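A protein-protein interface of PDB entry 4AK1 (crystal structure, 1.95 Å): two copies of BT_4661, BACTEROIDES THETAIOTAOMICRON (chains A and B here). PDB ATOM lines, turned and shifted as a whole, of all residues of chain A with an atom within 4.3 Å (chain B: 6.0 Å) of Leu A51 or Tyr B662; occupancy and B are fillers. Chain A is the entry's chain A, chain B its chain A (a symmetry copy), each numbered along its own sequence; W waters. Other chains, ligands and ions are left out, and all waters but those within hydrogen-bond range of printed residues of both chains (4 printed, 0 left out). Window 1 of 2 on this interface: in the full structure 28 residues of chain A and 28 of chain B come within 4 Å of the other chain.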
ATOM      1  N   THR A  50      17.398 -23.088 -10.794  1.00  0.00           N
ATOM      2  CA  THR A  50      18.754 -22.557 -10.601  1.00  0.00           C
ATOM      3  C   THR A  50      19.247 -22.909  -9.211  1.00  0.00           C
ATOM      4  O   THR A  50      18.440 -23.114  -8.293  1.00  0.00           O
ATOM      5  CB  THR A  50      18.852 -21.027 -10.807  1.00  0.00           C
ATOM      6  OG1 THR A  50      17.999 -20.353  -9.872  1.00  0.00           O
ATOM      7  CG2 THR A  50      18.460 -20.640 -12.234  1.00  0.00           C
ATOM      8  N   LEU A  51      20.562 -23.022  -9.069  1.00  0.00           N
ATOM      9  CA  LEU A  51      21.171 -23.224  -7.760  1.00  0.00           C
ATOM     10  C   LEU A  51      22.261 -22.178  -7.593  1.00  0.00           C
ATOM     11  O   LEU A  51      23.201 -22.120  -8.385  1.00  0.00           O
ATOM     12  CB  LEU A  51      21.739 -24.644  -7.619  1.00  0.00           C
ATOM     13  CG  LEU A  51      22.639 -24.931  -6.411  1.00  0.00           C
ATOM     14  CD1 LEU A  51      21.886 -24.726  -5.094  1.00  0.00           C
ATOM     15  CD2 LEU A  51      23.210 -26.343  -6.483  1.00  0.00           C
ATOM     16  N   ASP A  52      22.113 -21.325  -6.584  1.00  0.00           N
ATOM     17  CA  ASP A  52      23.142 -20.327  -6.270  1.00  0.00           C
ATOM     18  C   ASP A  52      23.490 -19.482  -7.516  1.00  0.00           C
ATOM     19  O   ASP A  52      24.657 -19.267  -7.837  1.00  0.00           O
ATOM     20  CB  ASP A  52      24.373 -21.052  -5.664  1.00  0.00           C
ATOM     21  CG  ASP A  52      25.490 -20.102  -5.233  1.00  0.00           C
ATOM     22  OD1 ASP A  52      25.202 -18.908  -4.988  1.00  0.00           O
ATOM     23  OD2 ASP A  52      26.657 -20.558  -5.136  1.00  0.00           O
ATOM     24  N   GLY A  53      22.457 -19.024  -8.222  1.00  0.00           N
ATOM     25  CA  GLY A  53      22.615 -18.139  -9.381  1.00  0.00           C
ATOM     26  C   GLY A  53      23.079 -18.782 -10.691  1.00  0.00           C
ATOM     27  O   GLY A  53      23.391 -18.069 -11.650  1.00  0.00           O
ATOM     28  N   GLU A  54      23.133 -20.114 -10.740  1.00  0.00           N
ATOM     29  CA  GLU A  54      23.548 -20.820 -11.956  1.00  0.00           C
ATOM     30  C   GLU A  54      22.557 -21.915 -12.325  1.00  0.00           C
ATOM     31  O   GLU A  54      21.879 -22.434 -11.447  1.00  0.00           O
ATOM     32  CB  GLU A  54      24.926 -21.455 -11.761  1.00  0.00           C
ATOM     33  CG  GLU A  54      26.034 -20.474 -11.433  1.00  0.00           C
ATOM     34  CD  GLU A  54      26.395 -19.555 -12.581  1.00  0.00           C
ATOM     35  OE1 GLU A  54      25.997 -19.799 -13.736  1.00  0.00           O
ATOM     36  OE2 GLU A  54      27.104 -18.576 -12.322  1.00  0.00           O
ATOM     37  N   PHE A  56      20.795 -25.356 -12.914  1.00  0.00           N
ATOM     38  CA  PHE A  56      20.909 -26.672 -12.304  1.00  0.00           C
ATOM     39  C   PHE A  56      20.325 -27.695 -13.281  1.00  0.00           C
ATOM     40  O   PHE A  56      19.125 -27.697 -13.557  1.00  0.00           O
ATOM     41  CB  PHE A  56      20.188 -26.714 -10.952  1.00  0.00           C
ATOM     42  CG  PHE A  56      20.418 -27.983 -10.189  1.00  0.00           C
ATOM     43  CD1 PHE A  56      21.513 -28.106  -9.333  1.00  0.00           C
ATOM     44  CD2 PHE A  56      19.553 -29.073 -10.334  1.00  0.00           C
ATOM     45  CE1 PHE A  56      21.735 -29.277  -8.633  1.00  0.00           C
ATOM     46  CE2 PHE A  56      19.785 -30.253  -9.643  1.00  0.00           C
ATOM     47  CZ  PHE A  56      20.870 -30.349  -8.785  1.00  0.00           C
ATOM     48  N   PRO A  79      23.112 -31.232  -3.940  1.00  0.00           N
ATOM     49  CA  PRO A  79      24.113 -30.306  -3.390  1.00  0.00           C
ATOM     50  C   PRO A  79      23.483 -29.204  -2.545  1.00  0.00           C
ATOM     51  O   PRO A  79      22.310 -28.860  -2.731  1.00  0.00           O
ATOM     52  CB  PRO A  79      24.794 -29.697  -4.631  1.00  0.00           C
ATOM     53  CG  PRO A  79      24.138 -30.305  -5.825  1.00  0.00           C
ATOM     54  CD  PRO A  79      22.948 -31.098  -5.401  1.00  0.00           C
ATOM     55  N   GLY A  81      22.565 -25.634  -1.008  1.00  0.00           N
ATOM     56  CA  GLY A  81      22.395 -24.230  -1.364  1.00  0.00           C
ATOM     57  C   GLY A  81      20.952 -23.866  -1.656  1.00  0.00           C
ATOM     58  O   GLY A  81      20.061 -24.706  -1.549  1.00  0.00           O
ATOM     59  N   LEU A  82      20.725 -22.613  -2.045  1.00  0.00           N
ATOM     60  CA  LEU A  82      19.378 -22.120  -2.342  1.00  0.00           C
ATOM     61  C   LEU A  82      18.970 -22.372  -3.798  1.00  0.00           C
ATOM     62  O   LEU A  82      19.629 -21.885  -4.723  1.00  0.00           O
ATOM     63  CB  LEU A  82      19.286 -20.630  -2.012  1.00  0.00           C
ATOM     64  CG  LEU A  82      17.963 -19.914  -2.319  1.00  0.00           C
ATOM     65  CD1 LEU A  82      16.799 -20.523  -1.545  1.00  0.00           C
ATOM     66  CD2 LEU A  82      18.115 -18.440  -1.973  1.00  0.00           C
ATOM     67  N   TYR A  83      17.897 -23.143  -3.978  1.00  0.00           N
ATOM     68  CA  TYR A  83      17.340 -23.462  -5.292  1.00  0.00           C
ATOM     69  C   TYR A  83      16.184 -22.523  -5.611  1.00  0.00           C
ATOM     70  O   TYR A  83      15.389 -22.186  -4.719  1.00  0.00           O
ATOM     71  CB  TYR A  83      16.828 -24.911  -5.342  1.00  0.00           C
ATOM     72  CG  TYR A  83      17.916 -25.972  -5.291  1.00  0.00           C
ATOM     73  CD1 TYR A  83      18.456 -26.386  -4.072  1.00  0.00           C
ATOM     74  CD2 TYR A  83      18.391 -26.571  -6.460  1.00  0.00           C
ATOM     75  CE1 TYR A  83      19.451 -27.355  -4.012  1.00  0.00           C
ATOM     76  CE2 TYR A  83      19.401 -27.536  -6.419  1.00  0.00           C
ATOM     77  CZ  TYR A  83      19.928 -27.925  -5.184  1.00  0.00           C
ATOM     78  OH  TYR A  83      20.920 -28.890  -5.116  1.00  0.00           O
ATOM     79  N   PRO B 556      31.803 -25.359 -13.045  1.00  0.00           N
ATOM     80  CA  PRO B 556      31.320 -26.360 -12.074  1.00  0.00           C
ATOM     81  C   PRO B 556      29.785 -26.426 -11.971  1.00  0.00           C
ATOM     82  O   PRO B 556      29.252 -27.396 -11.420  1.00  0.00           O
ATOM     83  CB  PRO B 556      31.918 -25.875 -10.749  1.00  0.00           C
ATOM     84  CG  PRO B 556      32.004 -24.396 -10.910  1.00  0.00           C
ATOM     85  CD  PRO B 556      32.359 -24.168 -12.366  1.00  0.00           C
ATOM     86  N   ALA B 557      29.086 -25.406 -12.475  1.00  0.00           N
ATOM     87  CA  ALA B 557      27.626 -25.447 -12.494  1.00  0.00           C
ATOM     88  C   ALA B 557      27.152 -26.362 -13.640  1.00  0.00           C
ATOM     89  O   ALA B 557      26.318 -27.246 -13.444  1.00  0.00           O
ATOM     90  CB  ALA B 557      27.038 -24.035 -12.629  1.00  0.00           C
ATOM     91  N   GLY B 591      37.830 -18.806  -4.907  1.00  0.00           N
ATOM     92  CA  GLY B 591      36.618 -19.269  -4.267  1.00  0.00           C
ATOM     93  C   GLY B 591      36.489 -18.785  -2.830  1.00  0.00           C
ATOM     94  O   GLY B 591      37.356 -18.060  -2.326  1.00  0.00           O
ATOM     95  N   PRO B 592      35.403 -19.205  -2.154  1.00  0.00           N
ATOM     96  CA  PRO B 592      35.168 -18.844  -0.767  1.00  0.00           C
ATOM     97  C   PRO B 592      36.310 -19.285   0.146  1.00  0.00           C
ATOM     98  O   PRO B 592      36.998 -20.271  -0.139  1.00  0.00           O
ATOM     99  CB  PRO B 592      33.891 -19.616  -0.421  1.00  0.00           C
ATOM    100  CG  PRO B 592      33.168 -19.720  -1.725  1.00  0.00           C
ATOM    101  CD  PRO B 592      34.277 -19.970  -2.720  1.00  0.00           C
ATOM    102  N   HIS B 595      36.731 -22.946   1.150  1.00  0.00           N
ATOM    103  CA  HIS B 595      37.285 -23.934   0.198  1.00  0.00           C
ATOM    104  C   HIS B 595      38.753 -24.133   0.487  1.00  0.00           C
ATOM    105  O   HIS B 595      39.614 -23.719  -0.281  1.00  0.00           O
ATOM    106  CB  HIS B 595      37.052 -23.473  -1.252  1.00  0.00           C
ATOM    107  CG  HIS B 595      35.592 -23.463  -1.664  1.00  0.00           C
ATOM    108  ND1 HIS B 595      35.196 -23.364  -2.960  1.00  0.00           N
ATOM    109  CD2 HIS B 595      34.419 -23.543  -0.898  1.00  0.00           C
ATOM    110  CE1 HIS B 595      33.844 -23.379  -3.014  1.00  0.00           C
ATOM    111  NE2 HIS B 595      33.373 -23.484  -1.753  1.00  0.00           N
ATOM    112  N   PHE B 607      38.604 -28.610   1.607  1.00  0.00           N
ATOM    113  CA  PHE B 607      37.601 -28.685   0.533  1.00  0.00           C
ATOM    114  C   PHE B 607      37.436 -30.123  -0.004  1.00  0.00           C
ATOM    115  O   PHE B 607      36.305 -30.600  -0.186  1.00  0.00           O
ATOM    116  CB  PHE B 607      37.878 -27.679  -0.594  1.00  0.00           C
ATOM    117  CG  PHE B 607      36.752 -27.567  -1.609  1.00  0.00           C
ATOM    118  CD1 PHE B 607      35.480 -27.150  -1.221  1.00  0.00           C
ATOM    119  CD2 PHE B 607      36.971 -27.867  -2.959  1.00  0.00           C
ATOM    120  CE1 PHE B 607      34.447 -27.057  -2.153  1.00  0.00           C
ATOM    121  CE2 PHE B 607      35.948 -27.759  -3.892  1.00  0.00           C
ATOM    122  CZ  PHE B 607      34.682 -27.346  -3.487  1.00  0.00           C
ATOM    123  N   ASN B 654      26.964 -29.214 -11.134  1.00  0.00           N
ATOM    124  CA  ASN B 654      26.534 -28.604  -9.868  1.00  0.00           C
ATOM    125  C   ASN B 654      27.088 -29.195  -8.568  1.00  0.00           C
ATOM    126  O   ASN B 654      26.653 -28.792  -7.496  1.00  0.00           O
ATOM    127  CB  ASN B 654      25.005 -28.500  -9.784  1.00  0.00           C
ATOM    128  CG  ASN B 654      24.410 -27.797 -10.986  1.00  0.00           C
ATOM    129  OD1 ASN B 654      23.885 -28.441 -11.891  1.00  0.00           O
ATOM    130  ND2 ASN B 654      24.497 -26.471 -11.002  1.00  0.00           N
ATOM    131  N   LEU B 655      28.016 -30.140  -8.661  1.00  0.00           N
ATOM    132  CA  LEU B 655      28.527 -30.839  -7.458  1.00  0.00           C
ATOM    133  C   LEU B 655      29.734 -30.156  -6.821  1.00  0.00           C
ATOM    134  O   LEU B 655      29.894 -30.169  -5.595  1.00  0.00           O
ATOM    135  CB  LEU B 655      28.859 -32.311  -7.784  1.00  0.00           C
ATOM    136  CG  LEU B 655      27.696 -33.150  -8.327  1.00  0.00           C
ATOM    137  CD1 LEU B 655      28.144 -34.585  -8.620  1.00  0.00           C
ATOM    138  CD2 LEU B 655      26.518 -33.104  -7.354  1.00  0.00           C
ATOM    139  N   TRP B 656      30.586 -29.564  -7.651  1.00  0.00           N
ATOM    140  CA  TRP B 656      31.790 -28.915  -7.133  1.00  0.00           C
ATOM    141  C   TRP B 656      31.490 -27.555  -6.528  1.00  0.00           C
ATOM    142  O   TRP B 656      31.592 -26.517  -7.182  1.00  0.00           O
ATOM    143  CB  TRP B 656      32.866 -28.875  -8.203  1.00  0.00           C
ATOM    144  CG  TRP B 656      33.418 -30.258  -8.459  1.00  0.00           C
ATOM    145  CD1 TRP B 656      32.909 -31.227  -9.312  1.00  0.00           C
ATOM    146  CD2 TRP B 656      34.593 -30.871  -7.831  1.00  0.00           C
ATOM    147  NE1 TRP B 656      33.685 -32.365  -9.274  1.00  0.00           N
ATOM    148  CE2 TRP B 656      34.700 -32.220  -8.395  1.00  0.00           C
ATOM    149  CE3 TRP B 656      35.530 -30.454  -6.881  1.00  0.00           C
ATOM    150  CZ2 TRP B 656      35.717 -33.092  -8.026  1.00  0.00           C
ATOM    151  CZ3 TRP B 656      36.548 -31.345  -6.517  1.00  0.00           C
ATOM    152  CH2 TRP B 656      36.645 -32.626  -7.085  1.00  0.00           C
ATOM    153  N   ARG B 657      31.113 -27.588  -5.255  1.00  0.00           N
ATOM    154  CA  ARG B 657      30.644 -26.436  -4.497  1.00  0.00           C
ATOM    155  C   ARG B 657      30.487 -26.819  -3.030  1.00  0.00           C
ATOM    156  O   ARG B 657      30.459 -28.001  -2.682  1.00  0.00           O
ATOM    157  CB  ARG B 657      29.275 -25.956  -5.024  1.00  0.00           C
ATOM    158  CG  ARG B 657      28.157 -27.001  -4.985  1.00  0.00           C
ATOM    159  CD  ARG B 657      26.783 -26.385  -5.320  1.00  0.00           C
ATOM    160  NE  ARG B 657      26.231 -25.541  -4.257  1.00  0.00           N
ATOM    161  CZ  ARG B 657      26.293 -24.203  -4.227  1.00  0.00           C
ATOM    162  NH1 ARG B 657      26.918 -23.525  -5.204  1.00  0.00           N
ATOM    163  NH2 ARG B 657      25.746 -23.529  -3.208  1.00  0.00           N
ATOM    164  N   ASN B 658      30.346 -25.821  -2.171  1.00  0.00           N
ATOM    165  CA  ASN B 658      29.738 -26.074  -0.861  1.00  0.00           C
ATOM    166  C   ASN B 658      28.699 -24.992  -0.556  1.00  0.00           C
ATOM    167  O   ASN B 658      28.318 -24.226  -1.453  1.00  0.00           O
ATOM    168  CB  ASN B 658      30.804 -26.228   0.243  1.00  0.00           C
ATOM    169  CG  ASN B 658      31.454 -24.905   0.640  1.00  0.00           C
ATOM    170  OD1 ASN B 658      31.195 -23.856   0.045  1.00  0.00           O
ATOM    171  ND2 ASN B 658      32.308 -24.957   1.662  1.00  0.00           N
ATOM    172  N   ASP B 660      28.948 -22.216   0.640  1.00  0.00           N
ATOM    173  CA  ASP B 660      29.431 -20.855   0.412  1.00  0.00           C
ATOM    174  C   ASP B 660      29.598 -20.475  -1.049  1.00  0.00           C
ATOM    175  O   ASP B 660      29.820 -19.308  -1.354  1.00  0.00           O
ATOM    176  CB  ASP B 660      30.735 -20.584   1.178  1.00  0.00           C
ATOM    177  CG  ASP B 660      30.529 -20.572   2.668  1.00  0.00           C
ATOM    178  OD1 ASP B 660      29.471 -20.092   3.113  1.00  0.00           O
ATOM    179  OD2 ASP B 660      31.404 -21.073   3.399  1.00  0.00           O
ATOM    180  N   GLY B 661      29.509 -21.446  -1.954  1.00  0.00           N
ATOM    181  CA  GLY B 661      29.592 -21.139  -3.366  1.00  0.00           C
ATOM    182  C   GLY B 661      30.275 -22.201  -4.201  1.00  0.00           C
ATOM    183  O   GLY B 661      30.788 -23.213  -3.670  1.00  0.00           O
ATOM    184  N   TYR B 662      30.265 -21.963  -5.512  1.00  0.00           N
ATOM    185  CA  TYR B 662      30.873 -22.881  -6.463  1.00  0.00           C
ATOM    186  C   TYR B 662      32.394 -22.859  -6.361  1.00  0.00           C
ATOM    187  O   TYR B 662      33.000 -21.820  -6.062  1.00  0.00           O
ATOM    188  CB  TYR B 662      30.441 -22.559  -7.908  1.00  0.00           C
ATOM    189  CG  TYR B 662      29.021 -23.006  -8.209  1.00  0.00           C
ATOM    190  CD1 TYR B 662      28.711 -24.355  -8.427  1.00  0.00           C
ATOM    191  CD2 TYR B 662      27.993 -22.078  -8.271  1.00  0.00           C
ATOM    192  CE1 TYR B 662      27.393 -24.756  -8.684  1.00  0.00           C
ATOM    193  CE2 TYR B 662      26.690 -22.469  -8.527  1.00  0.00           C
ATOM    194  CZ  TYR B 662      26.396 -23.799  -8.728  1.00  0.00           C
ATOM    195  OH  TYR B 662      25.077 -24.126  -8.989  1.00  0.00           O
ATOM    196  N   ALA B 663      33.008 -24.005  -6.635  1.00  0.00           N
ATOM    197  CA  ALA B 663      34.467 -24.104  -6.700  1.00  0.00           C
ATOM    198  C   ALA B 663      35.034 -23.062  -7.677  1.00  0.00           C
ATOM    199  O   ALA B 663      34.498 -22.840  -8.766  1.00  0.00           O
ATOM    200  CB  ALA B 663      34.886 -25.499  -7.154  1.00  0.00           C
ATOM    201  N   ASN B 664      36.132 -22.450  -7.271  1.00  0.00           N
ATOM    202  CA  ASN B 664      36.934 -21.599  -8.146  1.00  0.00           C
ATOM    203  C   ASN B 664      38.374 -21.891  -7.760  1.00  0.00           C
ATOM    204  O   ASN B 664      38.892 -21.354  -6.767  1.00  0.00           O
ATOM    205  CB  ASN B 664      36.588 -20.114  -7.953  1.00  0.00           C
ATOM    206  CG  ASN B 664      37.272 -19.219  -8.982  1.00  0.00           C
ATOM    207  OD1 ASN B 664      38.502 -19.122  -9.013  1.00  0.00           O
ATOM    208  ND2 ASN B 664      36.476 -18.562  -9.831  1.00  0.00           N
ATOM    209  N   THR B 698      33.125 -20.563 -12.743  1.00  0.00           N
ATOM    210  CA  THR B 698      31.834 -20.315 -13.370  1.00  0.00           C
ATOM    211  C   THR B 698      31.916 -19.319 -14.532  1.00  0.00           C
ATOM    212  O   THR B 698      30.966 -19.182 -15.269  1.00  0.00           O
ATOM    213  CB  THR B 698      30.774 -19.857 -12.357  1.00  0.00           C
ATOM    214  OG1 THR B 698      31.277 -18.739 -11.612  1.00  0.00           O
ATOM    215  CG2 THR B 698      30.431 -21.014 -11.393  1.00  0.00           C
HETATM  216  O   HOH W   1      25.943 -20.896  -2.032  1.00  0.00           O
HETATM  217  O   HOH W   2      29.201 -19.335  -6.159  1.00  0.00           O
HETATM  218  O   HOH W   3      28.309 -17.848 -10.326  1.00  0.00           O
HETATM  219  O   HOH W   4      26.956 -18.324  -2.542  1.00  0.00           O
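Water W3 bridges the side-chain carboxylate of Glu A54 (2.4 Å) and the side-chain hydroxyl of Thr B698 (3.4 Å).
Water W1 bridges NH2 of Arg B657 (2.9 Å) and OD2 of Asp A52 (3.2 Å).
Water W2 lies within hydrogen-bond range of N of Tyr B662 (2.9 Å) and OD2 of Asp A52 (3.0 Å).
Water W4 bridges the side-chain carboxylate (OD1) of Asp A52 (3.1 Å) and the backbone carbonyl oxygen (O) of Asp B660 (3.3 Å).
Of chain B, only Arg B657 and Tyr B662 come within 4 Å of Leu A51.
Tyr A83 touches none of the printed residues of chain B.
Of the printed residues of chain A, Asn B654 touches Phe A56 (3.3 Å) and Pro A79 (3.4 Å).
Asn B658 touches none of the printed residues of chain A.
Of the printed residues of chain A, Gly B661 touches Asp A52.
Of the printed residues of chain A, Tyr B662 touches Leu A51, Asp A52 and Glu A54.
The nearest printed residue of chain B that does not touch Glu A54 is Asn B654 (4.8 Å).
The side-chain carboxylate (OD2) of Asp A52 is in salt-bridge range of the guanidinium group (NH1) of Arg B657 (3.0 Å).
OH of Tyr B662 is in hydrogen-bond range of O of Leu A51, at 2.8 Å.
Among the printed residues, pairs that only touch across the chains: Leu A51 with Arg B657, Asp A52 with Gly B661, Asp A52 with Tyr B662, Glu A54 with Ala B557, Glu A54 with Tyr B662, Glu A54 with Thr B698, Phe A56 with Asn B654, Pro A79 with Asn B654, Pro A79 with Leu B655, Pro A79 with Arg B657 and Gly A81 with Arg B657.
No position is printed for both chains.
Of the 13 pairs that touch across the chains among the printed residues, none has its exchanged pair printed and touching as well.
Hydrophobic or aromatic side chains of chain B within 4 Å of the printed part of chain A: Ala B557, Leu B655 and Tyr B662.
Among the printed residues, Asp or Glu carboxylates within 4 Å of a Lys or Arg side-chain nitrogen of the other chain: Asp A52 with Arg B657 (3.0 Å).
The backbone carbonyl oxygen (O) of Pro A79 is in hydrogen-bond range of the side-chain hydroxyl (OH) of Tyr A83.
The side-chain amide nitrogen (ND2) of Asn B654 sits at hydrogen-bond distance from the side-chain hydroxyl (OH) of Tyr B662 (3.1 Å).
O of Leu A82 is in hydrogen-bond range of N of Asp A52, at 3.2 Å.
The backbone carbonyl oxygen of Pro B556 sits at hydrogen-bond distance from the backbone NH of Asn B654, 2.9 Å away.
The backbone NH (N) of Asn B654 is in hydrogen-bond range of the backbone carbonyl oxygen (O) of Ala B557, 3.1 Å away.
A ring nitrogen (NE2) of His B595 sits close to the backbone carbonyl oxygen (O) of Gly B661 (3.2 Å).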
